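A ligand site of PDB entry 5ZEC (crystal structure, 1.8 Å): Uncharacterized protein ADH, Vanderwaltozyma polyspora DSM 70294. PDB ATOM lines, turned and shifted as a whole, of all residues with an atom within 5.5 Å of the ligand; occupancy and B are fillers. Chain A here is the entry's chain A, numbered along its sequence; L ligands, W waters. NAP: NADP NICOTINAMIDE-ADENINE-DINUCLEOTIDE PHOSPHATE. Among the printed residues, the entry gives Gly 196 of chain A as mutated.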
ATOM      1  N   GLY A   7       3.631  10.365 -31.636  1.00  0.00           N
ATOM      2  CA  GLY A   7       3.508   9.047 -31.018  1.00  0.00           C
ATOM      3  C   GLY A   7       2.140   8.813 -30.406  1.00  0.00           C
ATOM      4  O   GLY A   7       2.012   8.391 -29.244  1.00  0.00           O
ATOM      5  N   ALA A   8       1.103   9.056 -31.198  1.00  0.00           N
ATOM      6  CA  ALA A   8      -0.266   9.118 -30.697  1.00  0.00           C
ATOM      7  C   ALA A   8      -0.919   7.755 -30.543  1.00  0.00           C
ATOM      8  O   ALA A   8      -2.060   7.701 -30.059  1.00  0.00           O
ATOM      9  CB  ALA A   8      -1.116  10.010 -31.616  1.00  0.00           C
ATOM     10  N   SER A   9      -0.249   6.668 -30.931  1.00  0.00           N
ATOM     11  CA  SER A   9      -0.818   5.329 -30.787  1.00  0.00           C
ATOM     12  C   SER A   9      -0.440   4.664 -29.468  1.00  0.00           C
ATOM     13  O   SER A   9      -0.938   3.567 -29.181  1.00  0.00           O
ATOM     14  CB  SER A   9      -0.385   4.433 -31.959  1.00  0.00           C
ATOM     15  OG  SER A   9       1.022   4.272 -31.965  1.00  0.00           O
ATOM     16  N   GLY A  10       0.410   5.319 -28.662  1.00  0.00           N
ATOM     17  CA  GLY A  10       0.914   4.690 -27.458  1.00  0.00           C
ATOM     18  C   GLY A  10      -0.061   4.682 -26.296  1.00  0.00           C
ATOM     19  O   GLY A  10      -1.156   5.260 -26.347  1.00  0.00           O
ATOM     20  N   TYR A  11       0.368   4.003 -25.238  1.00  0.00           N
ATOM     21  CA  TYR A  11      -0.428   3.807 -24.023  1.00  0.00           C
ATOM     22  C   TYR A  11      -0.779   5.143 -23.382  1.00  0.00           C
ATOM     23  O   TYR A  11      -1.963   5.457 -23.165  1.00  0.00           O
ATOM     24  CB  TYR A  11       0.388   2.919 -23.080  1.00  0.00           C
ATOM     25  CG  TYR A  11      -0.072   2.842 -21.657  1.00  0.00           C
ATOM     26  CD1 TYR A  11       0.826   3.075 -20.619  1.00  0.00           C
ATOM     27  CD2 TYR A  11      -1.382   2.502 -21.323  1.00  0.00           C
ATOM     28  CE1 TYR A  11       0.436   2.966 -19.292  1.00  0.00           C
ATOM     29  CE2 TYR A  11      -1.795   2.405 -19.973  1.00  0.00           C
ATOM     30  CZ  TYR A  11      -0.865   2.636 -18.975  1.00  0.00           C
ATOM     31  OH  TYR A  11      -1.226   2.534 -17.640  1.00  0.00           O
ATOM     32  N   ILE A  12       0.225   5.960 -23.093  1.00  0.00           N
ATOM     33  CA  ILE A  12      -0.025   7.274 -22.499  1.00  0.00           C
ATOM     34  C   ILE A  12      -0.737   8.191 -23.490  1.00  0.00           C
ATOM     35  O   ILE A  12      -1.712   8.872 -23.150  1.00  0.00           O
ATOM     36  CB  ILE A  12       1.290   7.890 -21.996  1.00  0.00           C
ATOM     37  CG1 ILE A  12       1.880   7.042 -20.869  1.00  0.00           C
ATOM     38  CG2 ILE A  12       1.077   9.329 -21.513  1.00  0.00           C
ATOM     39  CD1 ILE A  12       3.315   7.445 -20.488  1.00  0.00           C
ATOM     40  N   ALA A  13      -0.264   8.215 -24.744  1.00  0.00           N
ATOM     41  CA  ALA A  13      -0.787   9.181 -25.705  1.00  0.00           C
ATOM     42  C   ALA A  13      -2.270   8.961 -26.002  1.00  0.00           C
ATOM     43  O   ALA A  13      -3.005   9.923 -26.274  1.00  0.00           O
ATOM     44  CB  ALA A  13       0.048   9.115 -26.995  1.00  0.00           C
ATOM     45  N   THR A  30       0.480  11.850 -34.641  1.00  0.00           N
ATOM     46  CA  THR A  30       1.389  11.188 -35.585  1.00  0.00           C
ATOM     47  C   THR A  30       1.515   9.728 -35.207  1.00  0.00           C
ATOM     48  O   THR A  30       1.660   9.394 -34.024  1.00  0.00           O
ATOM     49  CB  THR A  30       2.779  11.856 -35.651  1.00  0.00           C
ATOM     50  OG1 THR A  30       3.648  11.352 -34.631  1.00  0.00           O
ATOM     51  CG2 THR A  30       2.666  13.388 -35.561  1.00  0.00           C
ATOM     52  N   ARG A  32       2.950   5.662 -36.911  1.00  0.00           N
ATOM     53  CA  ARG A  32       3.938   5.104 -37.827  1.00  0.00           C
ATOM     54  C   ARG A  32       3.356   4.591 -39.135  1.00  0.00           C
ATOM     55  O   ARG A  32       4.095   4.507 -40.124  1.00  0.00           O
ATOM     56  CB  ARG A  32       4.689   3.958 -37.153  1.00  0.00           C
ATOM     57  CG  ARG A  32       5.745   4.366 -36.128  1.00  0.00           C
ATOM     58  CD  ARG A  32       6.737   3.212 -36.090  1.00  0.00           C
ATOM     59  NE  ARG A  32       7.551   3.079 -34.888  1.00  0.00           N
ATOM     60  CZ  ARG A  32       8.873   3.168 -34.863  1.00  0.00           C
ATOM     61  NH1 ARG A  32       9.526   2.989 -33.724  1.00  0.00           N
ATOM     62  NH2 ARG A  32       9.559   3.464 -35.963  1.00  0.00           N
ATOM     63  N   LYS A  36      -2.349   1.838 -38.339  1.00  0.00           N
ATOM     64  CA  LYS A  36      -2.627   2.333 -36.991  1.00  0.00           C
ATOM     65  C   LYS A  36      -3.523   3.561 -37.036  1.00  0.00           C
ATOM     66  O   LYS A  36      -4.451   3.682 -36.226  1.00  0.00           O
ATOM     67  CB  LYS A  36      -1.311   2.627 -36.268  1.00  0.00           C
ATOM     68  CG  LYS A  36      -0.467   1.383 -36.076  1.00  0.00           C
ATOM     69  CD  LYS A  36       0.890   1.656 -35.415  1.00  0.00           C
ATOM     70  CE  LYS A  36       1.595   0.332 -35.087  1.00  0.00           C
ATOM     71  NZ  LYS A  36       3.056   0.472 -34.842  1.00  0.00           N
ATOM     72  N   VAL A  54       4.159   9.551 -39.528  1.00  0.00           N
ATOM     73  CA  VAL A  54       5.583   9.743 -39.319  1.00  0.00           C
ATOM     74  C   VAL A  54       6.190   8.390 -38.996  1.00  0.00           C
ATOM     75  O   VAL A  54       6.147   7.936 -37.851  1.00  0.00           O
ATOM     76  CB  VAL A  54       5.860  10.754 -38.190  1.00  0.00           C
ATOM     77  CG1 VAL A  54       7.356  10.855 -37.908  1.00  0.00           C
ATOM     78  CG2 VAL A  54       5.297  12.112 -38.554  1.00  0.00           C
ATOM     79  N   PRO A  55       6.732   7.692 -39.995  1.00  0.00           N
ATOM     80  CA  PRO A  55       7.152   6.289 -39.772  1.00  0.00           C
ATOM     81  C   PRO A  55       8.329   6.152 -38.826  1.00  0.00           C
ATOM     82  O   PRO A  55       8.473   5.107 -38.185  1.00  0.00           O
ATOM     83  CB  PRO A  55       7.528   5.801 -41.182  1.00  0.00           C
ATOM     84  CG  PRO A  55       6.976   6.815 -42.128  1.00  0.00           C
ATOM     85  CD  PRO A  55       6.888   8.116 -41.389  1.00  0.00           C
ATOM     86  N   GLU A  56       9.175   7.171 -38.721  1.00  0.00           N
ATOM     87  CA  GLU A  56      10.436   7.030 -37.988  1.00  0.00           C
ATOM     88  C   GLU A  56      10.864   8.416 -37.513  1.00  0.00           C
ATOM     89  O   GLU A  56      11.283   9.240 -38.332  1.00  0.00           O
ATOM     90  CB  GLU A  56      11.494   6.392 -38.870  1.00  0.00           C
ATOM     91  CG  GLU A  56      12.847   6.242 -38.186  1.00  0.00           C
ATOM     92  CD  GLU A  56      12.701   5.580 -36.829  1.00  0.00           C
ATOM     93  OE1 GLU A  56      12.397   4.363 -36.801  1.00  0.00           O
ATOM     94  OE2 GLU A  56      12.857   6.285 -35.795  1.00  0.00           O
ATOM     95  N   ILE A  57      10.744   8.677 -36.206  1.00  0.00           N
ATOM     96  CA  ILE A  57      11.067  10.018 -35.726  1.00  0.00           C
ATOM     97  C   ILE A  57      12.562  10.318 -35.851  1.00  0.00           C
ATOM     98  O   ILE A  57      12.952  11.478 -35.875  1.00  0.00           O
ATOM     99  CB  ILE A  57      10.617  10.228 -34.257  1.00  0.00           C
ATOM    100  CG1 ILE A  57      11.385   9.296 -33.312  1.00  0.00           C
ATOM    101  CG2 ILE A  57       9.101  10.070 -34.126  1.00  0.00           C
ATOM    102  CD1 ILE A  57      10.872   9.351 -31.861  1.00  0.00           C
ATOM    103  N   ALA A  58      13.399   9.284 -35.966  1.00  0.00           N
ATOM    104  CA  ALA A  58      14.844   9.494 -36.063  1.00  0.00           C
ATOM    105  C   ALA A  58      15.287  10.012 -37.422  1.00  0.00           C
ATOM    106  O   ALA A  58      16.390  10.560 -37.527  1.00  0.00           O
ATOM    107  CB  ALA A  58      15.580   8.187 -35.750  1.00  0.00           C
ATOM    108  N   ALA A  80       5.402  13.385 -27.384  1.00  0.00           N
ATOM    109  CA  ALA A  80       5.359  12.182 -26.561  1.00  0.00           C
ATOM    110  C   ALA A  80       6.055  10.979 -27.187  1.00  0.00           C
ATOM    111  O   ALA A  80       6.162   9.944 -26.516  1.00  0.00           O
ATOM    112  CB  ALA A  80       3.893  11.821 -26.252  1.00  0.00           C
ATOM    113  N   ALA A  81       6.555  11.072 -28.421  1.00  0.00           N
ATOM    114  CA  ALA A  81       7.137   9.923 -29.107  1.00  0.00           C
ATOM    115  C   ALA A  81       8.598   9.710 -28.687  1.00  0.00           C
ATOM    116  O   ALA A  81       9.460  10.541 -28.962  1.00  0.00           O
ATOM    117  CB  ALA A  81       7.052  10.100 -30.620  1.00  0.00           C
ATOM    118  N   SER A  82       8.867   8.568 -28.057  1.00  0.00           N
ATOM    119  CA  SER A  82      10.222   8.117 -27.757  1.00  0.00           C
ATOM    120  C   SER A  82      10.149   6.617 -27.563  1.00  0.00           C
ATOM    121  O   SER A  82       9.121   6.120 -27.112  1.00  0.00           O
ATOM    122  CB  SER A  82      10.774   8.797 -26.486  1.00  0.00           C
ATOM    123  OG  SER A  82      12.191   8.736 -26.437  1.00  0.00           O
ATOM    124  N   PRO A  83      11.195   5.869 -27.939  1.00  0.00           N
ATOM    125  CA  PRO A  83      11.118   4.401 -27.847  1.00  0.00           C
ATOM    126  C   PRO A  83      11.053   3.889 -26.416  1.00  0.00           C
ATOM    127  O   PRO A  83      11.833   4.302 -25.553  1.00  0.00           O
ATOM    128  CB  PRO A  83      12.395   3.933 -28.552  1.00  0.00           C
ATOM    129  CG  PRO A  83      13.246   5.098 -28.691  1.00  0.00           C
ATOM    130  CD  PRO A  83      12.353   6.310 -28.721  1.00  0.00           C
ATOM    131  N   VAL A  84      10.105   2.988 -26.176  1.00  0.00           N
ATOM    132  CA  VAL A  84      10.079   2.207 -24.955  1.00  0.00           C
ATOM    133  C   VAL A  84      10.443   0.746 -25.205  1.00  0.00           C
ATOM    134  O   VAL A  84      11.058   0.103 -24.336  1.00  0.00           O
ATOM    135  CB  VAL A  84       8.701   2.312 -24.254  1.00  0.00           C
ATOM    136  CG1 VAL A  84       8.603   1.311 -23.126  1.00  0.00           C
ATOM    137  CG2 VAL A  84       8.520   3.723 -23.702  1.00  0.00           C
ATOM    138  N   ASN A  85      10.152   0.209 -26.383  1.00  0.00           N
ATOM    139  CA  ASN A  85      10.627  -1.105 -26.800  1.00  0.00           C
ATOM    140  C   ASN A  85      11.812  -0.931 -27.742  1.00  0.00           C
ATOM    141  O   ASN A  85      11.868   0.025 -28.522  1.00  0.00           O
ATOM    142  CB  ASN A  85       9.498  -1.860 -27.504  1.00  0.00           C
ATOM    143  CG  ASN A  85       8.221  -1.888 -26.679  1.00  0.00           C
ATOM    144  OD1 ASN A  85       8.245  -2.258 -25.506  1.00  0.00           O
ATOM    145  ND2 ASN A  85       7.119  -1.458 -27.285  1.00  0.00           N
ATOM    146  N   PRO A  98      16.749   7.573 -31.723  1.00  0.00           N
ATOM    147  CA  PRO A  98      15.391   8.080 -31.947  1.00  0.00           C
ATOM    148  C   PRO A  98      14.909   9.018 -30.852  1.00  0.00           C
ATOM    149  O   PRO A  98      14.162   9.959 -31.124  1.00  0.00           O
ATOM    150  CB  PRO A  98      14.529   6.817 -32.039  1.00  0.00           C
ATOM    151  CG  PRO A  98      15.519   5.713 -32.418  1.00  0.00           C
ATOM    152  CD  PRO A  98      16.804   6.095 -31.717  1.00  0.00           C
ATOM    153  N   THR A 124       7.152  14.726 -23.123  1.00  0.00           N
ATOM    154  CA  THR A 124       7.193  13.596 -22.170  1.00  0.00           C
ATOM    155  C   THR A 124       8.652  13.207 -21.961  1.00  0.00           C
ATOM    156  O   THR A 124       9.271  12.580 -22.817  1.00  0.00           O
ATOM    157  CB  THR A 124       6.398  12.407 -22.681  1.00  0.00           C
ATOM    158  OG1 THR A 124       5.175  12.842 -23.291  1.00  0.00           O
ATOM    159  CG2 THR A 124       6.083  11.454 -21.497  1.00  0.00           C
ATOM    160  N   ALA A 125       9.207  13.631 -20.828  1.00  0.00           N
ATOM    161  CA  ALA A 125      10.518  13.133 -20.420  1.00  0.00           C
ATOM    162  C   ALA A 125      10.250  11.927 -19.528  1.00  0.00           C
ATOM    163  O   ALA A 125       9.382  11.114 -19.843  1.00  0.00           O
ATOM    164  CB  ALA A 125      11.342  14.209 -19.708  1.00  0.00           C
ATOM    165  N   SER A 126      10.945  11.828 -18.399  1.00  0.00           N
ATOM    166  CA  SER A 126      10.729  10.668 -17.539  1.00  0.00           C
ATOM    167  C   SER A 126      11.307  10.955 -16.171  1.00  0.00           C
ATOM    168  O   SER A 126      12.240  11.744 -16.033  1.00  0.00           O
ATOM    169  CB  SER A 126      11.388   9.409 -18.119  1.00  0.00           C
ATOM    170  OG  SER A 126      11.237   8.298 -17.229  1.00  0.00           O
ATOM    171  N   TYR A 127      10.758  10.273 -15.171  1.00  0.00           N
ATOM    172  CA  TYR A 127      11.470  10.181 -13.898  1.00  0.00           C
ATOM    173  C   TYR A 127      12.912   9.753 -14.148  1.00  0.00           C
ATOM    174  O   TYR A 127      13.819  10.145 -13.406  1.00  0.00           O
ATOM    175  CB  TYR A 127      10.708   9.180 -13.009  1.00  0.00           C
ATOM    176  CG  TYR A 127      11.320   8.797 -11.691  1.00  0.00           C
ATOM    177  CD1 TYR A 127      11.812   9.759 -10.817  1.00  0.00           C
ATOM    178  CD2 TYR A 127      11.332   7.474 -11.276  1.00  0.00           C
ATOM    179  CE1 TYR A 127      12.344   9.398  -9.585  1.00  0.00           C
ATOM    180  CE2 TYR A 127      11.853   7.106 -10.042  1.00  0.00           C
ATOM    181  CZ  TYR A 127      12.351   8.079  -9.203  1.00  0.00           C
ATOM    182  OH  TYR A 127      12.884   7.731  -7.970  1.00  0.00           O
ATOM    183  N   TYR A 164      18.024   3.072 -21.539  1.00  0.00           N
ATOM    184  CA  TYR A 164      16.749   3.765 -21.693  1.00  0.00           C
ATOM    185  C   TYR A 164      16.716   5.044 -20.865  1.00  0.00           C
ATOM    186  O   TYR A 164      16.221   6.074 -21.343  1.00  0.00           O
ATOM    187  CB  TYR A 164      15.568   2.860 -21.301  1.00  0.00           C
ATOM    188  CG  TYR A 164      14.283   3.642 -21.226  1.00  0.00           C
ATOM    189  CD1 TYR A 164      13.511   3.877 -22.371  1.00  0.00           C
ATOM    190  CD2 TYR A 164      13.845   4.200 -20.023  1.00  0.00           C
ATOM    191  CE1 TYR A 164      12.342   4.605 -22.307  1.00  0.00           C
ATOM    192  CE2 TYR A 164      12.678   4.941 -19.941  1.00  0.00           C
ATOM    193  CZ  TYR A 164      11.931   5.148 -21.093  1.00  0.00           C
ATOM    194  OH  TYR A 164      10.772   5.879 -20.984  1.00  0.00           O
ATOM    195  N   LYS A 168      16.244   9.097 -22.307  1.00  0.00           N
ATOM    196  CA  LYS A 168      15.346  10.158 -21.846  1.00  0.00           C
ATOM    197  C   LYS A 168      16.138  11.373 -21.374  1.00  0.00           C
ATOM    198  O   LYS A 168      15.763  12.520 -21.658  1.00  0.00           O
ATOM    199  CB  LYS A 168      14.448   9.624 -20.744  1.00  0.00           C
ATOM    200  CG  LYS A 168      13.646   8.419 -21.173  1.00  0.00           C
ATOM    201  CD  LYS A 168      12.687   8.752 -22.338  1.00  0.00           C
ATOM    202  CE  LYS A 168      11.544   9.678 -21.912  1.00  0.00           C
ATOM    203  NZ  LYS A 168      10.672  10.071 -23.090  1.00  0.00           N
ATOM    204  N   HIS A 194       7.648  14.181 -16.164  1.00  0.00           N
ATOM    205  CA  HIS A 194       8.592  13.144 -15.755  1.00  0.00           C
ATOM    206  C   HIS A 194       7.870  12.049 -14.976  1.00  0.00           C
ATOM    207  O   HIS A 194       7.946  11.994 -13.749  1.00  0.00           O
ATOM    208  CB  HIS A 194       9.722  13.742 -14.909  1.00  0.00           C
ATOM    209  CG  HIS A 194      10.469  14.850 -15.602  1.00  0.00           C
ATOM    210  ND1 HIS A 194      11.736  14.681 -16.110  1.00  0.00           N
ATOM    211  CD2 HIS A 194      10.110  16.118 -15.888  1.00  0.00           C
ATOM    212  CE1 HIS A 194      12.147  15.812 -16.668  1.00  0.00           C
ATOM    213  NE2 HIS A 194      11.176  16.701 -16.542  1.00  0.00           N
ATOM    214  N   PRO A 195       7.173  11.135 -15.662  1.00  0.00           N
ATOM    215  CA  PRO A 195       6.459  10.070 -14.964  1.00  0.00           C
ATOM    216  C   PRO A 195       7.389   8.978 -14.440  1.00  0.00           C
ATOM    217  O   PRO A 195       8.393   8.639 -15.061  1.00  0.00           O
ATOM    218  CB  PRO A 195       5.540   9.486 -16.051  1.00  0.00           C
ATOM    219  CG  PRO A 195       5.532  10.540 -17.164  1.00  0.00           C
ATOM    220  CD  PRO A 195       6.892  11.139 -17.110  1.00  0.00           C
ATOM    221  N   GLY A 196       7.015   8.412 -13.291  1.00  0.00           N
ATOM    222  CA  GLY A 196       7.617   7.161 -12.864  1.00  0.00           C
ATOM    223  C   GLY A 196       7.042   6.030 -13.696  1.00  0.00           C
ATOM    224  O   GLY A 196       6.473   6.287 -14.751  1.00  0.00           O
ATOM    225  N   PHE A 197       7.136   4.782 -13.238  1.00  0.00           N
ATOM    226  CA  PHE A 197       6.506   3.688 -13.958  1.00  0.00           C
ATOM    227  C   PHE A 197       5.007   3.940 -14.075  1.00  0.00           C
ATOM    228  O   PHE A 197       4.332   4.114 -13.051  1.00  0.00           O
ATOM    229  CB  PHE A 197       6.764   2.346 -13.253  1.00  0.00           C
ATOM    230  CG  PHE A 197       8.044   1.698 -13.665  1.00  0.00           C
ATOM    231  CD1 PHE A 197       8.035   0.697 -14.634  1.00  0.00           C
ATOM    232  CD2 PHE A 197       9.249   2.094 -13.115  1.00  0.00           C
ATOM    233  CE1 PHE A 197       9.218   0.102 -15.026  1.00  0.00           C
ATOM    234  CE2 PHE A 197      10.438   1.491 -13.497  1.00  0.00           C
ATOM    235  CZ  PHE A 197      10.422   0.488 -14.453  1.00  0.00           C
ATOM    236  N   VAL A 198       4.479   3.945 -15.297  1.00  0.00           N
ATOM    237  CA  VAL A 198       3.089   4.329 -15.511  1.00  0.00           C
ATOM    238  C   VAL A 198       2.207   3.095 -15.538  1.00  0.00           C
ATOM    239  O   VAL A 198       2.403   2.187 -16.353  1.00  0.00           O
ATOM    240  CB  VAL A 198       2.929   5.144 -16.807  1.00  0.00           C
ATOM    241  CG1 VAL A 198       1.444   5.528 -16.966  1.00  0.00           C
ATOM    242  CG2 VAL A 198       3.838   6.391 -16.765  1.00  0.00           C
ATOM    243  N   THR A 215       4.886  -0.807 -19.732  1.00  0.00           N
ATOM    244  CA  THR A 215       5.030  -0.968 -18.292  1.00  0.00           C
ATOM    245  C   THR A 215       3.868  -1.735 -17.659  1.00  0.00           C
ATOM    246  O   THR A 215       4.047  -2.374 -16.613  1.00  0.00           O
ATOM    247  CB  THR A 215       5.179   0.410 -17.640  1.00  0.00           C
ATOM    248  OG1 THR A 215       4.190   1.298 -18.193  1.00  0.00           O
ATOM    249  CG2 THR A 215       6.570   0.961 -17.942  1.00  0.00           C
HETATM  250  PA  NAP L   1       4.291   3.219 -25.930  1.00  0.00           P
HETATM  251  O1A NAP L   1       2.890   2.645 -25.811  1.00  0.00           O
HETATM  252  O2A NAP L   1       5.268   2.234 -26.565  1.00  0.00           O
HETATM  253  O5B NAP L   1       4.163   4.614 -26.778  1.00  0.00           O
HETATM  254  C5B NAP L   1       5.305   5.053 -27.481  1.00  0.00           C
HETATM  255  C4B NAP L   1       4.824   5.871 -28.716  1.00  0.00           C
HETATM  256  O4B NAP L   1       5.849   6.442 -29.336  1.00  0.00           O
HETATM  257  C3B NAP L   1       4.167   4.937 -29.751  1.00  0.00           C
HETATM  258  O3B NAP L   1       3.185   5.577 -30.447  1.00  0.00           O
HETATM  259  C2B NAP L   1       5.372   4.624 -30.657  1.00  0.00           C
HETATM  260  O2B NAP L   1       4.855   4.168 -31.958  1.00  0.00           O
HETATM  261  C1B NAP L   1       6.006   5.778 -30.789  1.00  0.00           C
HETATM  262  N9A NAP L   1       7.411   5.636 -31.057  1.00  0.00           N
HETATM  263  C8A NAP L   1       8.447   5.199 -30.319  1.00  0.00           C
HETATM  264  N7A NAP L   1       9.558   5.264 -31.056  1.00  0.00           N
HETATM  265  C5A NAP L   1       9.209   5.752 -32.245  1.00  0.00           C
HETATM  266  C6A NAP L   1       9.960   6.023 -33.364  1.00  0.00           C
HETATM  267  N6A NAP L   1      11.374   5.798 -33.454  1.00  0.00           N
HETATM  268  N1A NAP L   1       9.401   6.498 -34.469  1.00  0.00           N
HETATM  269  C2A NAP L   1       8.074   6.742 -34.484  1.00  0.00           C
HETATM  270  N3A NAP L   1       7.315   6.482 -33.392  1.00  0.00           N
HETATM  271  C4A NAP L   1       7.886   5.990 -32.267  1.00  0.00           C
HETATM  272  O3  NAP L   1       4.906   3.554 -24.475  1.00  0.00           O
HETATM  273  PN  NAP L   1       4.374   4.697 -23.445  1.00  0.00           P
HETATM  274  O1N NAP L   1       4.563   4.075 -22.081  1.00  0.00           O
HETATM  275  O2N NAP L   1       2.991   5.132 -23.801  1.00  0.00           O
HETATM  276  O5D NAP L   1       5.460   5.930 -23.578  1.00  0.00           O
HETATM  277  C5D NAP L   1       5.103   7.102 -24.232  1.00  0.00           C
HETATM  278  C4D NAP L   1       6.068   8.216 -23.731  1.00  0.00           C
HETATM  279  O4D NAP L   1       6.032   8.221 -22.411  1.00  0.00           O
HETATM  280  C3D NAP L   1       7.535   7.982 -24.130  1.00  0.00           C
HETATM  281  O3D NAP L   1       8.173   9.179 -24.398  1.00  0.00           O
HETATM  282  C2D NAP L   1       8.094   7.345 -22.835  1.00  0.00           C
HETATM  283  O2D NAP L   1       9.558   7.459 -22.823  1.00  0.00           O
HETATM  284  C1D NAP L   1       7.531   8.083 -21.883  1.00  0.00           C
HETATM  285  N1N NAP L   1       7.454   7.523 -20.543  1.00  0.00           N
HETATM  286  C2N NAP L   1       6.796   6.371 -20.296  1.00  0.00           C
HETATM  287  C3N NAP L   1       6.738   5.867 -19.012  1.00  0.00           C
HETATM  288  C7N NAP L   1       6.032   4.553 -18.728  1.00  0.00           C
HETATM  289  O7N NAP L   1       5.343   3.940 -19.496  1.00  0.00           O
HETATM  290  N7N NAP L   1       6.248   4.052 -17.432  1.00  0.00           N
HETATM  291  C4N NAP L   1       7.356   6.538 -17.987  1.00  0.00           C
HETATM  292  C5N NAP L   1       8.002   7.697 -18.232  1.00  0.00           C
HETATM  293  C6N NAP L   1       8.039   8.194 -19.519  1.00  0.00           C
HETATM  294  P2B NAP L   1       4.915   2.562 -32.306  1.00  0.00           P
HETATM  295  O1X NAP L   1       4.211   2.405 -33.635  1.00  0.00           O
HETATM  296  O2X NAP L   1       4.302   1.728 -31.212  1.00  0.00           O
HETATM  297  O3X NAP L   1       6.377   2.173 -32.438  1.00  0.00           O
HETATM  298  O   HOH W   1       4.467   6.913 -33.662  1.00  0.00           O
HETATM  299  O   HOH W   2       4.127  -0.826 -31.427  1.00  0.00           O
HETATM  300  O   HOH W   3       8.683  12.298 -25.591  1.00  0.00           O
HETATM  301  O   HOH W   4       2.801   0.427 -24.121  1.00  0.00           O
HETATM  302  O   HOH W   5       8.047   1.640 -30.203  1.00  0.00           O
HETATM  303  O   HOH W   6       3.737   8.491 -27.141  1.00  0.00           O
HETATM  304  O   HOH W   7       8.014   2.440 -27.917  1.00  0.00           O
HETATM  305  O   HOH W   8       5.750   0.969 -28.820  1.00  0.00           O
HETATM  306  O   HOH W   9       6.822  -0.101 -33.957  1.00  0.00           O
HETATM  307  O   HOH W  10      12.599   3.214 -32.001  1.00  0.00           O
HETATM  308  O   HOH W  11       1.783   2.179 -30.532  1.00  0.00           O
HETATM  309  O   HOH W  12       5.390  -0.238 -25.402  1.00  0.00           O
HETATM  310  O   HOH W  13       4.178   1.416 -21.729  1.00  0.00           O
HETATM  311  O   HOH W  14       2.675   4.602 -34.142  1.00  0.00           O
HETATM  312  O   HOH W  15       2.024   6.947 -25.537  1.00  0.00           O
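The backbone NH of Val 198 sits close to a nitrogen (N7N) of the ligand, 2.8 Å away.
Merely in contact with the ligand: Ala 81 (3.7 Å), Ser 82 (3.4 Å), Pro 83 (3.6 Å), Val 84 (3.7 Å), Pro 98 (3.6 Å), Thr 124 (3.4 Å), Ala 125 (3.2 Å), Ser 126 (3.4 Å), Pro 195 (3.3 Å) and Phe 197 (3.5 Å).
Hydrophobic or aromatic side chains that line the ligand: Tyr 11, Ile 12, Ile 57, Pro 83, Val 84, Pro 98, Tyr 164, Pro 195 and Val 198.
Of the 34 residues printed, 25 come within 4 Å of the ligand.
The nearest printed residue that does not touch the ligand is Val 54 (4.1 Å).
Water W8 lies within hydrogen-bond range of O2A of the ligand (2.6 Å) and ND2 of Asn 85 (3.2 Å).
Water W13 lies within hydrogen-bond range of O1N of the ligand (2.7 Å) and N of Thr 215 (3.1 Å).
Water W12 lies within hydrogen-bond range of O2A of the ligand (2.7 Å) and ND2 of Asn 85 (2.8 Å).
Water W9 lies within hydrogen-bond range of O3X of the ligand and NE of Arg 32.
Water W7 lies within hydrogen-bond range of N of Val 84, O2A of the ligand and N of Asn 85.
Water W6 bridges O of Gly 7 (2.7 Å) and O of Ala 80 (2.9 Å).
The backbone carbonyl oxygen of Val 198 is in hydrogen-bond range of the side-chain hydroxyl of Thr 215 (2.7 Å).
OE1 of Glu 56 lies within salt-bridge range of NH2 of Arg 32 (3.1 Å).
OE2 of Glu 56 lies within hydrogen-bond range of N of Ala 58, at 3.1 Å.
NZ of Lys 168 is in hydrogen-bond range of O of Thr 124 (2.9 Å).
The backbone carbonyl oxygen (O) of Pro 55 sits at hydrogen-bond distance from the guanidinium group (NH2) of Arg 32 (3.0 Å).
N of Gly 7 is in hydrogen-bond range of OG1 of Thr 30.
The backbone carbonyl oxygen (O) of Pro 195 lies within hydrogen-bond range of the backbone NH (N) of Tyr 127, at 2.9 Å.
O of Ser 126 is in hydrogen-bond range of ND1 of His 194 (3.0 Å).
O1X of the ligand lies within salt-bridge range of NZ of Lys 36.
An oxygen (O2D) of the ligand sits at hydrogen-bond distance from the side-chain hydroxyl of Tyr 164.
N6A of the ligand sits at hydrogen-bond distance from OE2 of Glu 56, 2.8 Å away.
The side-chain amino group (NZ) of Lys 168 sits at hydrogen-bond distance from an oxygen (O2D) of the ligand, at 2.9 Å.
The guanidinium group of Arg 32 lies within salt-bridge range of an oxygen (O3X) of the ligand, 2.9 Å away.
The backbone NH (N) of Tyr 11 is in hydrogen-bond range of an oxygen (O1A) of the ligand, 2.9 Å away.
The side-chain hydroxyl of Ser 9 lies within hydrogen-bond range of an oxygen (O3B) of the ligand, 2.9 Å away.
The backbone NH (N) of Ile 12 lies within hydrogen-bond range of an oxygen (O2N) of the ligand (3.0 Å).
The backbone carbonyl oxygen of Ala 80 lies within hydrogen-bond range of an oxygen (O3D) of the ligand, at 3.0 Å.
The backbone NH (N) of Ile 57 sits at hydrogen-bond distance from a nitrogen (N1A) of the ligand (3.1 Å).
The side-chain hydroxyl (OG1) of Thr 215 is in hydrogen-bond range of an oxygen (O7N) of the ligand (3.2 Å).
O of Gly 7 is in hydrogen-bond range of O3B of the ligand (3.3 Å).
The backbone NH of Gly 10 is in hydrogen-bond range of an oxygen (O3B) of the ligand (3.3 Å).
N7N of the ligand sits close to O of Gly 196, 3.5 Å away.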
